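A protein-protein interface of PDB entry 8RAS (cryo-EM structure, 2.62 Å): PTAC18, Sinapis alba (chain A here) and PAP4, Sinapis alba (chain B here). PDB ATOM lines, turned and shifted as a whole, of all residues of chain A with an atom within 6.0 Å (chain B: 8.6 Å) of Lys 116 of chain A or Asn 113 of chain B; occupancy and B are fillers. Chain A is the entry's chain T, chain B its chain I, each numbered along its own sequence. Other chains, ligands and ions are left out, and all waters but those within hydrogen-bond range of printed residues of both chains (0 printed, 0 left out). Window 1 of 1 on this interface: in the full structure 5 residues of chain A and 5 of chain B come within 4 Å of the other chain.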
ATOM      1  N   ASN A  46      10.700 -35.649   2.267  1.00  0.00           N
ATOM      2  CA  ASN A  46      11.308 -35.528   0.942  1.00  0.00           C
ATOM      3  C   ASN A  46      12.671 -36.225   0.901  1.00  0.00           C
ATOM      4  O   ASN A  46      13.721 -35.605   0.720  1.00  0.00           O
ATOM      5  CB  ASN A  46      11.413 -34.056   0.524  1.00  0.00           C
ATOM      6  CG  ASN A  46      12.036 -33.877  -0.847  1.00  0.00           C
ATOM      7  OD1 ASN A  46      12.811 -32.948  -1.072  1.00  0.00           O
ATOM      8  ND2 ASN A  46      11.699 -34.768  -1.772  1.00  0.00           N
ATOM      9  N   TRP A  80      21.317 -31.529   7.795  1.00  0.00           N
ATOM     10  CA  TRP A  80      21.738 -31.472   6.396  1.00  0.00           C
ATOM     11  C   TRP A  80      21.400 -30.102   5.836  1.00  0.00           C
ATOM     12  O   TRP A  80      20.321 -29.881   5.290  1.00  0.00           O
ATOM     13  CB  TRP A  80      21.063 -32.565   5.581  1.00  0.00           C
ATOM     14  CG  TRP A  80      21.640 -33.909   5.795  1.00  0.00           C
ATOM     15  CD1 TRP A  80      22.528 -34.561   4.995  1.00  0.00           C
ATOM     16  CD2 TRP A  80      21.374 -34.776   6.895  1.00  0.00           C
ATOM     17  NE1 TRP A  80      22.827 -35.791   5.530  1.00  0.00           N
ATOM     18  CE2 TRP A  80      22.130 -35.945   6.699  1.00  0.00           C
ATOM     19  CE3 TRP A  80      20.563 -34.679   8.028  1.00  0.00           C
ATOM     20  CZ2 TRP A  80      22.101 -37.006   7.594  1.00  0.00           C
ATOM     21  CZ3 TRP A  80      20.537 -35.730   8.914  1.00  0.00           C
ATOM     22  CH2 TRP A  80      21.300 -36.877   8.693  1.00  0.00           C
ATOM     23  N   GLN A  81      22.335 -29.169   5.960  1.00  0.00           N
ATOM     24  CA  GLN A  81      22.187 -27.890   5.283  1.00  0.00           C
ATOM     25  C   GLN A  81      22.709 -27.927   3.854  1.00  0.00           C
ATOM     26  O   GLN A  81      22.706 -26.891   3.180  1.00  0.00           O
ATOM     27  CB  GLN A  81      22.873 -26.786   6.093  1.00  0.00           C
ATOM     28  CG  GLN A  81      24.339 -27.027   6.374  1.00  0.00           C
ATOM     29  CD  GLN A  81      24.755 -26.497   7.736  1.00  0.00           C
ATOM     30  OE1 GLN A  81      23.947 -26.437   8.661  1.00  0.00           O
ATOM     31  NE2 GLN A  81      26.018 -26.110   7.861  1.00  0.00           N
ATOM     32  N   VAL A  82      23.161 -29.090   3.385  1.00  0.00           N
ATOM     33  CA  VAL A  82      23.478 -29.332   1.985  1.00  0.00           C
ATOM     34  C   VAL A  82      22.877 -30.675   1.591  1.00  0.00           C
ATOM     35  O   VAL A  82      22.746 -31.582   2.419  1.00  0.00           O
ATOM     36  CB  VAL A  82      25.003 -29.322   1.714  1.00  0.00           C
ATOM     37  CG1 VAL A  82      25.281 -29.264   0.224  1.00  0.00           C
ATOM     38  CG2 VAL A  82      25.680 -28.160   2.426  1.00  0.00           C
ATOM     39  N   ASP A  83      22.498 -30.799   0.320  1.00  0.00           N
ATOM     40  CA  ASP A  83      22.037 -32.078  -0.201  1.00  0.00           C
ATOM     41  C   ASP A  83      23.187 -33.079  -0.246  1.00  0.00           C
ATOM     42  O   ASP A  83      24.354 -32.713  -0.405  1.00  0.00           O
ATOM     43  CB  ASP A  83      21.443 -31.907  -1.599  1.00  0.00           C
ATOM     44  CG  ASP A  83      20.056 -31.298  -1.574  1.00  0.00           C
ATOM     45  OD1 ASP A  83      19.308 -31.558  -0.608  1.00  0.00           O
ATOM     46  OD2 ASP A  83      19.711 -30.564  -2.523  1.00  0.00           O
ATOM     47  N   TYR A 114      19.712 -37.344   1.019  1.00  0.00           N
ATOM     48  CA  TYR A 114      19.228 -36.600   2.175  1.00  0.00           C
ATOM     49  C   TYR A 114      18.969 -35.147   1.790  1.00  0.00           C
ATOM     50  O   TYR A 114      19.864 -34.485   1.254  1.00  0.00           O
ATOM     51  CB  TYR A 114      20.232 -36.676   3.321  1.00  0.00           C
ATOM     52  CG  TYR A 114      20.309 -38.045   3.955  1.00  0.00           C
ATOM     53  CD1 TYR A 114      19.211 -38.594   4.599  1.00  0.00           C
ATOM     54  CD2 TYR A 114      21.478 -38.793   3.900  1.00  0.00           C
ATOM     55  CE1 TYR A 114      19.273 -39.847   5.177  1.00  0.00           C
ATOM     56  CE2 TYR A 114      21.550 -40.047   4.475  1.00  0.00           C
ATOM     57  CZ  TYR A 114      20.446 -40.569   5.111  1.00  0.00           C
ATOM     58  OH  TYR A 114      20.512 -41.817   5.686  1.00  0.00           O
ATOM     59  N   PRO A 115      17.776 -34.623   2.046  1.00  0.00           N
ATOM     60  CA  PRO A 115      17.444 -33.269   1.598  1.00  0.00           C
ATOM     61  C   PRO A 115      18.105 -32.197   2.451  1.00  0.00           C
ATOM     62  O   PRO A 115      18.520 -32.425   3.588  1.00  0.00           O
ATOM     63  CB  PRO A 115      15.921 -33.221   1.745  1.00  0.00           C
ATOM     64  CG  PRO A 115      15.645 -34.141   2.882  1.00  0.00           C
ATOM     65  CD  PRO A 115      16.678 -35.237   2.812  1.00  0.00           C
ATOM     66  N   LYS A 116      18.190 -31.005   1.869  1.00  0.00           N
ATOM     67  CA  LYS A 116      18.703 -29.847   2.584  1.00  0.00           C
ATOM     68  C   LYS A 116      17.742 -29.445   3.700  1.00  0.00           C
ATOM     69  O   LYS A 116      16.524 -29.618   3.594  1.00  0.00           O
ATOM     70  CB  LYS A 116      18.919 -28.683   1.615  1.00  0.00           C
ATOM     71  CG  LYS A 116      19.504 -27.426   2.234  1.00  0.00           C
ATOM     72  CD  LYS A 116      19.904 -26.431   1.160  1.00  0.00           C
ATOM     73  CE  LYS A 116      20.200 -25.061   1.747  1.00  0.00           C
ATOM     74  NZ  LYS A 116      21.410 -25.065   2.613  1.00  0.00           N
ATOM     75  N   TRP A 117      18.312 -28.925   4.789  1.00  0.00           N
ATOM     76  CA  TRP A 117      17.614 -28.461   5.988  1.00  0.00           C
ATOM     77  C   TRP A 117      17.009 -29.596   6.803  1.00  0.00           C
ATOM     78  O   TRP A 117      16.239 -29.333   7.735  1.00  0.00           O
ATOM     79  CB  TRP A 117      16.518 -27.441   5.660  1.00  0.00           C
ATOM     80  CG  TRP A 117      17.033 -26.184   5.048  1.00  0.00           C
ATOM     81  CD1 TRP A 117      18.073 -25.422   5.489  1.00  0.00           C
ATOM     82  CD2 TRP A 117      16.531 -25.539   3.873  1.00  0.00           C
ATOM     83  NE1 TRP A 117      18.250 -24.339   4.664  1.00  0.00           N
ATOM     84  CE2 TRP A 117      17.315 -24.388   3.663  1.00  0.00           C
ATOM     85  CE3 TRP A 117      15.495 -25.822   2.979  1.00  0.00           C
ATOM     86  CZ2 TRP A 117      17.095 -23.522   2.596  1.00  0.00           C
ATOM     87  CZ3 TRP A 117      15.279 -24.962   1.923  1.00  0.00           C
ATOM     88  CH2 TRP A 117      16.074 -23.825   1.739  1.00  0.00           C
ATOM     89  N   LEU A 118      17.332 -30.848   6.489  1.00  0.00           N
ATOM     90  CA  LEU A 118      16.792 -31.965   7.250  1.00  0.00           C
ATOM     91  C   LEU A 118      17.425 -32.016   8.635  1.00  0.00           C
ATOM     92  O   LEU A 118      18.650 -31.960   8.774  1.00  0.00           O
ATOM     93  CB  LEU A 118      17.032 -33.280   6.512  1.00  0.00           C
ATOM     94  CG  LEU A 118      16.682 -34.552   7.288  1.00  0.00           C
ATOM     95  CD1 LEU A 118      15.202 -34.583   7.635  1.00  0.00           C
ATOM     96  CD2 LEU A 118      17.078 -35.793   6.505  1.00  0.00           C
ATOM     97  N   TYR A 137      23.467 -26.489  -5.253  1.00  0.00           N
ATOM     98  CA  TYR A 137      22.320 -26.217  -6.105  1.00  0.00           C
ATOM     99  C   TYR A 137      22.637 -26.607  -7.545  1.00  0.00           C
ATOM    100  O   TYR A 137      23.786 -26.543  -7.989  1.00  0.00           O
ATOM    101  CB  TYR A 137      21.938 -24.738  -6.031  1.00  0.00           C
ATOM    102  CG  TYR A 137      20.739 -24.378  -6.877  1.00  0.00           C
ATOM    103  CD1 TYR A 137      20.732 -23.229  -7.652  1.00  0.00           C
ATOM    104  CD2 TYR A 137      19.602 -25.177  -6.878  1.00  0.00           C
ATOM    105  CE1 TYR A 137      19.636 -22.899  -8.425  1.00  0.00           C
ATOM    106  CE2 TYR A 137      18.502 -24.852  -7.647  1.00  0.00           C
ATOM    107  CZ  TYR A 137      18.525 -23.711  -8.417  1.00  0.00           C
ATOM    108  OH  TYR A 137      17.431 -23.379  -9.183  1.00  0.00           O
ATOM    109  N   LYS B 106       4.256 -25.172  -6.944  1.00  0.00           N
ATOM    110  CA  LYS B 106       4.548 -24.950  -5.532  1.00  0.00           C
ATOM    111  C   LYS B 106       5.125 -26.200  -4.880  1.00  0.00           C
ATOM    112  O   LYS B 106       6.042 -26.109  -4.056  1.00  0.00           O
ATOM    113  CB  LYS B 106       3.285 -24.495  -4.805  1.00  0.00           C
ATOM    114  CG  LYS B 106       3.094 -22.990  -4.782  1.00  0.00           C
ATOM    115  CD  LYS B 106       2.202 -22.559  -3.630  1.00  0.00           C
ATOM    116  CE  LYS B 106       2.812 -22.931  -2.289  1.00  0.00           C
ATOM    117  NZ  LYS B 106       2.369 -22.011  -1.206  1.00  0.00           N
ATOM    118  N   ALA B 107       4.595 -27.375  -5.227  1.00  0.00           N
ATOM    119  CA  ALA B 107       5.102 -28.613  -4.645  1.00  0.00           C
ATOM    120  C   ALA B 107       6.540 -28.881  -5.072  1.00  0.00           C
ATOM    121  O   ALA B 107       7.375 -29.273  -4.249  1.00  0.00           O
ATOM    122  CB  ALA B 107       4.201 -29.786  -5.031  1.00  0.00           C
ATOM    123  N   THR B 108       6.850 -28.673  -6.353  1.00  0.00           N
ATOM    124  CA  THR B 108       8.202 -28.919  -6.838  1.00  0.00           C
ATOM    125  C   THR B 108       9.181 -27.841  -6.395  1.00  0.00           C
ATOM    126  O   THR B 108      10.393 -28.077  -6.425  1.00  0.00           O
ATOM    127  CB  THR B 108       8.209 -29.030  -8.362  1.00  0.00           C
ATOM    128  OG1 THR B 108       7.406 -27.987  -8.925  1.00  0.00           O
ATOM    129  CG2 THR B 108       7.656 -30.377  -8.796  1.00  0.00           C
ATOM    130  N   TYR B 109       8.689 -26.667  -5.993  1.00  0.00           N
ATOM    131  CA  TYR B 109       9.579 -25.643  -5.455  1.00  0.00           C
ATOM    132  C   TYR B 109      10.207 -26.100  -4.144  1.00  0.00           C
ATOM    133  O   TYR B 109      11.374 -25.798  -3.869  1.00  0.00           O
ATOM    134  CB  TYR B 109       8.821 -24.332  -5.265  1.00  0.00           C
ATOM    135  CG  TYR B 109       9.679 -23.209  -4.734  1.00  0.00           C
ATOM    136  CD1 TYR B 109      10.765 -22.741  -5.459  1.00  0.00           C
ATOM    137  CD2 TYR B 109       9.403 -22.616  -3.510  1.00  0.00           C
ATOM    138  CE1 TYR B 109      11.554 -21.717  -4.982  1.00  0.00           C
ATOM    139  CE2 TYR B 109      10.187 -21.588  -3.025  1.00  0.00           C
ATOM    140  CZ  TYR B 109      11.262 -21.144  -3.764  1.00  0.00           C
ATOM    141  OH  TYR B 109      12.050 -20.123  -3.286  1.00  0.00           O
ATOM    142  N   ASN B 110       9.441 -26.821  -3.322  1.00  0.00           N
ATOM    143  CA  ASN B 110       9.951 -27.473  -2.115  1.00  0.00           C
ATOM    144  C   ASN B 110      10.583 -26.470  -1.150  1.00  0.00           C
ATOM    145  O   ASN B 110      11.640 -26.722  -0.570  1.00  0.00           O
ATOM    146  CB  ASN B 110      10.941 -28.585  -2.475  1.00  0.00           C
ATOM    147  CG  ASN B 110      11.177 -29.552  -1.333  1.00  0.00           C
ATOM    148  OD1 ASN B 110      10.541 -29.462  -0.284  1.00  0.00           O
ATOM    149  ND2 ASN B 110      12.099 -30.487  -1.534  1.00  0.00           N
ATOM    150  N   ASN B 111       9.924 -25.323  -0.981  1.00  0.00           N
ATOM    151  CA  ASN B 111      10.311 -24.319   0.013  1.00  0.00           C
ATOM    152  C   ASN B 111      11.763 -23.874  -0.166  1.00  0.00           C
ATOM    153  O   ASN B 111      12.553 -23.848   0.780  1.00  0.00           O
ATOM    154  CB  ASN B 111      10.069 -24.840   1.431  1.00  0.00           C
ATOM    155  CG  ASN B 111       9.771 -23.729   2.416  1.00  0.00           C
ATOM    156  OD1 ASN B 111       9.296 -22.659   2.037  1.00  0.00           O
ATOM    157  ND2 ASN B 111      10.047 -23.979   3.690  1.00  0.00           N
ATOM    158  N   GLY B 112      12.114 -23.520  -1.398  1.00  0.00           N
ATOM    159  CA  GLY B 112      13.441 -23.028  -1.699  1.00  0.00           C
ATOM    160  C   GLY B 112      14.476 -24.086  -2.005  1.00  0.00           C
ATOM    161  O   GLY B 112      15.656 -23.747  -2.154  1.00  0.00           O
ATOM    162  N   ASN B 113      14.077 -25.350  -2.108  1.00  0.00           N
ATOM    163  CA  ASN B 113      14.974 -26.448  -2.465  1.00  0.00           C
ATOM    164  C   ASN B 113      14.348 -27.205  -3.630  1.00  0.00           C
ATOM    165  O   ASN B 113      13.870 -28.334  -3.473  1.00  0.00           O
ATOM    166  CB  ASN B 113      15.219 -27.366  -1.267  1.00  0.00           C
ATOM    167  CG  ASN B 113      16.281 -28.409  -1.539  1.00  0.00           C
ATOM    168  OD1 ASN B 113      17.098 -28.260  -2.447  1.00  0.00           O
ATOM    169  ND2 ASN B 113      16.274 -29.477  -0.750  1.00  0.00           N
ATOM    170  N   PRO B 114      14.346 -26.605  -4.821  1.00  0.00           N
ATOM    171  CA  PRO B 114      13.506 -27.118  -5.912  1.00  0.00           C
ATOM    172  C   PRO B 114      13.830 -28.555  -6.290  1.00  0.00           C
ATOM    173  O   PRO B 114      14.990 -28.970  -6.317  1.00  0.00           O
ATOM    174  CB  PRO B 114      13.808 -26.157  -7.068  1.00  0.00           C
ATOM    175  CG  PRO B 114      14.297 -24.914  -6.412  1.00  0.00           C
ATOM    176  CD  PRO B 114      15.052 -25.372  -5.204  1.00  0.00           C
ATOM    177  N   LEU B 115      12.775 -29.312  -6.583  1.00  0.00           N
ATOM    178  CA  LEU B 115      12.915 -30.648  -7.128  1.00  0.00           C
ATOM    179  C   LEU B 115      13.354 -30.565  -8.588  1.00  0.00           C
ATOM    180  O   LEU B 115      13.246 -29.509  -9.216  1.00  0.00           O
ATOM    181  CB  LEU B 115      11.592 -31.402  -7.003  1.00  0.00           C
ATOM    182  CG  LEU B 115      11.079 -31.647  -5.582  1.00  0.00           C
ATOM    183  CD1 LEU B 115       9.902 -32.608  -5.594  1.00  0.00           C
ATOM    184  CD2 LEU B 115      12.190 -32.173  -4.692  1.00  0.00           C
ATOM    185  N   PRO B 116      13.870 -31.662  -9.150  1.00  0.00           N
ATOM    186  CA  PRO B 116      14.292 -31.625 -10.561  1.00  0.00           C
ATOM    187  C   PRO B 116      13.176 -31.260 -11.524  1.00  0.00           C
ATOM    188  O   PRO B 116      13.464 -30.752 -12.615  1.00  0.00           O
ATOM    189  CB  PRO B 116      14.804 -33.049 -10.816  1.00  0.00           C
ATOM    190  CG  PRO B 116      15.159 -33.574  -9.475  1.00  0.00           C
ATOM    191  CD  PRO B 116      14.207 -32.946  -8.509  1.00  0.00           C
ATOM    192  N   GLU B 117      11.917 -31.501 -11.162  1.00  0.00           N
ATOM    193  CA  GLU B 117      10.792 -31.197 -12.036  1.00  0.00           C
ATOM    194  C   GLU B 117      10.366 -29.735 -11.985  1.00  0.00           C
ATOM    195  O   GLU B 117       9.509 -29.334 -12.779  1.00  0.00           O
ATOM    196  CB  GLU B 117       9.597 -32.083 -11.678  1.00  0.00           C
ATOM    197  CG  GLU B 117       9.762 -33.544 -12.061  1.00  0.00           C
ATOM    198  CD  GLU B 117      10.575 -34.329 -11.048  1.00  0.00           C
ATOM    199  OE1 GLU B 117      10.989 -33.742 -10.027  1.00  0.00           O
ATOM    200  OE2 GLU B 117      10.799 -35.538 -11.274  1.00  0.00           O
ATOM    201  N   PHE B 118      10.934 -28.936 -11.077  1.00  0.00           N
ATOM    202  CA  PHE B 118      10.485 -27.555 -10.925  1.00  0.00           C
ATOM    203  C   PHE B 118      10.785 -26.722 -12.164  1.00  0.00           C
ATOM    204  O   PHE B 118       9.955 -25.909 -12.585  1.00  0.00           O
ATOM    205  CB  PHE B 118      11.131 -26.922  -9.693  1.00  0.00           C
ATOM    206  CG  PHE B 118      10.834 -25.457  -9.543  1.00  0.00           C
ATOM    207  CD1 PHE B 118       9.599 -25.031  -9.086  1.00  0.00           C
ATOM    208  CD2 PHE B 118      11.787 -24.506  -9.863  1.00  0.00           C
ATOM    209  CE1 PHE B 118       9.321 -23.684  -8.950  1.00  0.00           C
ATOM    210  CE2 PHE B 118      11.516 -23.158  -9.728  1.00  0.00           C
ATOM    211  CZ  PHE B 118      10.281 -22.747  -9.271  1.00  0.00           C
ATOM    212  N   ILE B 197      11.614 -19.295 -11.634  1.00  0.00           N
ATOM    213  CA  ILE B 197      10.733 -19.061 -10.498  1.00  0.00           C
ATOM    214  C   ILE B 197       9.673 -18.033 -10.873  1.00  0.00           C
ATOM    215  O   ILE B 197       9.944 -17.066 -11.598  1.00  0.00           O
ATOM    216  CB  ILE B 197      11.553 -18.616  -9.275  1.00  0.00           C
ATOM    217  CG1 ILE B 197      12.338 -19.797  -8.706  1.00  0.00           C
ATOM    218  CG2 ILE B 197      10.658 -18.048  -8.187  1.00  0.00           C
ATOM    219  CD1 ILE B 197      13.372 -19.401  -7.679  1.00  0.00           C
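Lys 116 of chain A touches just one residue of chain B: Asn 113 (3.6 Å). Of the printed residues of chain B, Asp 83 of chain A touches Asn 113. Printed residues of chain A within 4 Å of Leu 115 of chain B: Asn 46 (3.8 Å). Of the printed residues of chain A, Asn 110 of chain B touches Asn 46. Of the printed residues of chain A, Asn 111 of chain B touches Trp 117. Of the printed residues of chain A, Gly 112 of chain B touches Trp 117 (3.9 Å). Tyr 109 of chain B touches none of the printed residues of chain A. The nearest residue of chain B that does not touch Lys 116 of chain A is Gly 112 of chain B (6.0 Å). The nearest printed residue of chain A that does not touch Asn 113 of chain B is Pro 115 of chain A (4.5 Å). The nearest printed residue of chain B that does not touch Trp 117 of chain A is Asn 110 of chain B (4.7 Å).
ND2 of Asn 110 of chain B sits at hydrogen-bond distance from OD1 of Asn 46 of chain A, 2.6 Å away. The side-chain amide oxygen (OD1) of Asn 113 of chain B sits close to the side-chain carboxylate (OD2) of Asp 83 of chain A (3.5 Å).
Hydrophobic or aromatic side chains of chain B that line the printed part of chain A: Leu 115. Of the 11 printed residues of chain A, 4 touch a printed residue of chain B. Printed residues of chain A that touch a printed residue of chain B: Asn 46, Asp 83, Lys 116 and Trp 117. Hydrophobic or aromatic side chains of chain A that line the printed part of chain B: Trp 117. Among the printed residues, 7 pairs touch across the chains. Among the printed residues, no Asp or Glu carboxylate lies within 4 Å of a Lys or Arg side-chain nitrogen of the other chain.
Among the printed residues, pairs that only touch across the chains: Asn 46 of chain A with Leu 115 of chain B, Lys 116 of chain A with Asn 113 of chain B, Trp 117 of chain A with Asn 111 of chain B, Trp 117 of chain A with Gly 112 of chain B and Trp 117 of chain A with Asn 113 of chain B.
O of Thr 108 of chain B is in hydrogen-bond range of N of Leu 115 of chain B. ND2 of Asn 110 of chain B lies close to O of Asn 113 of chain B. The backbone NH of Lys 116 of chain A is in hydrogen-bond range of the side-chain carboxylate of Asp 83 of chain A, at 2.8 Å.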
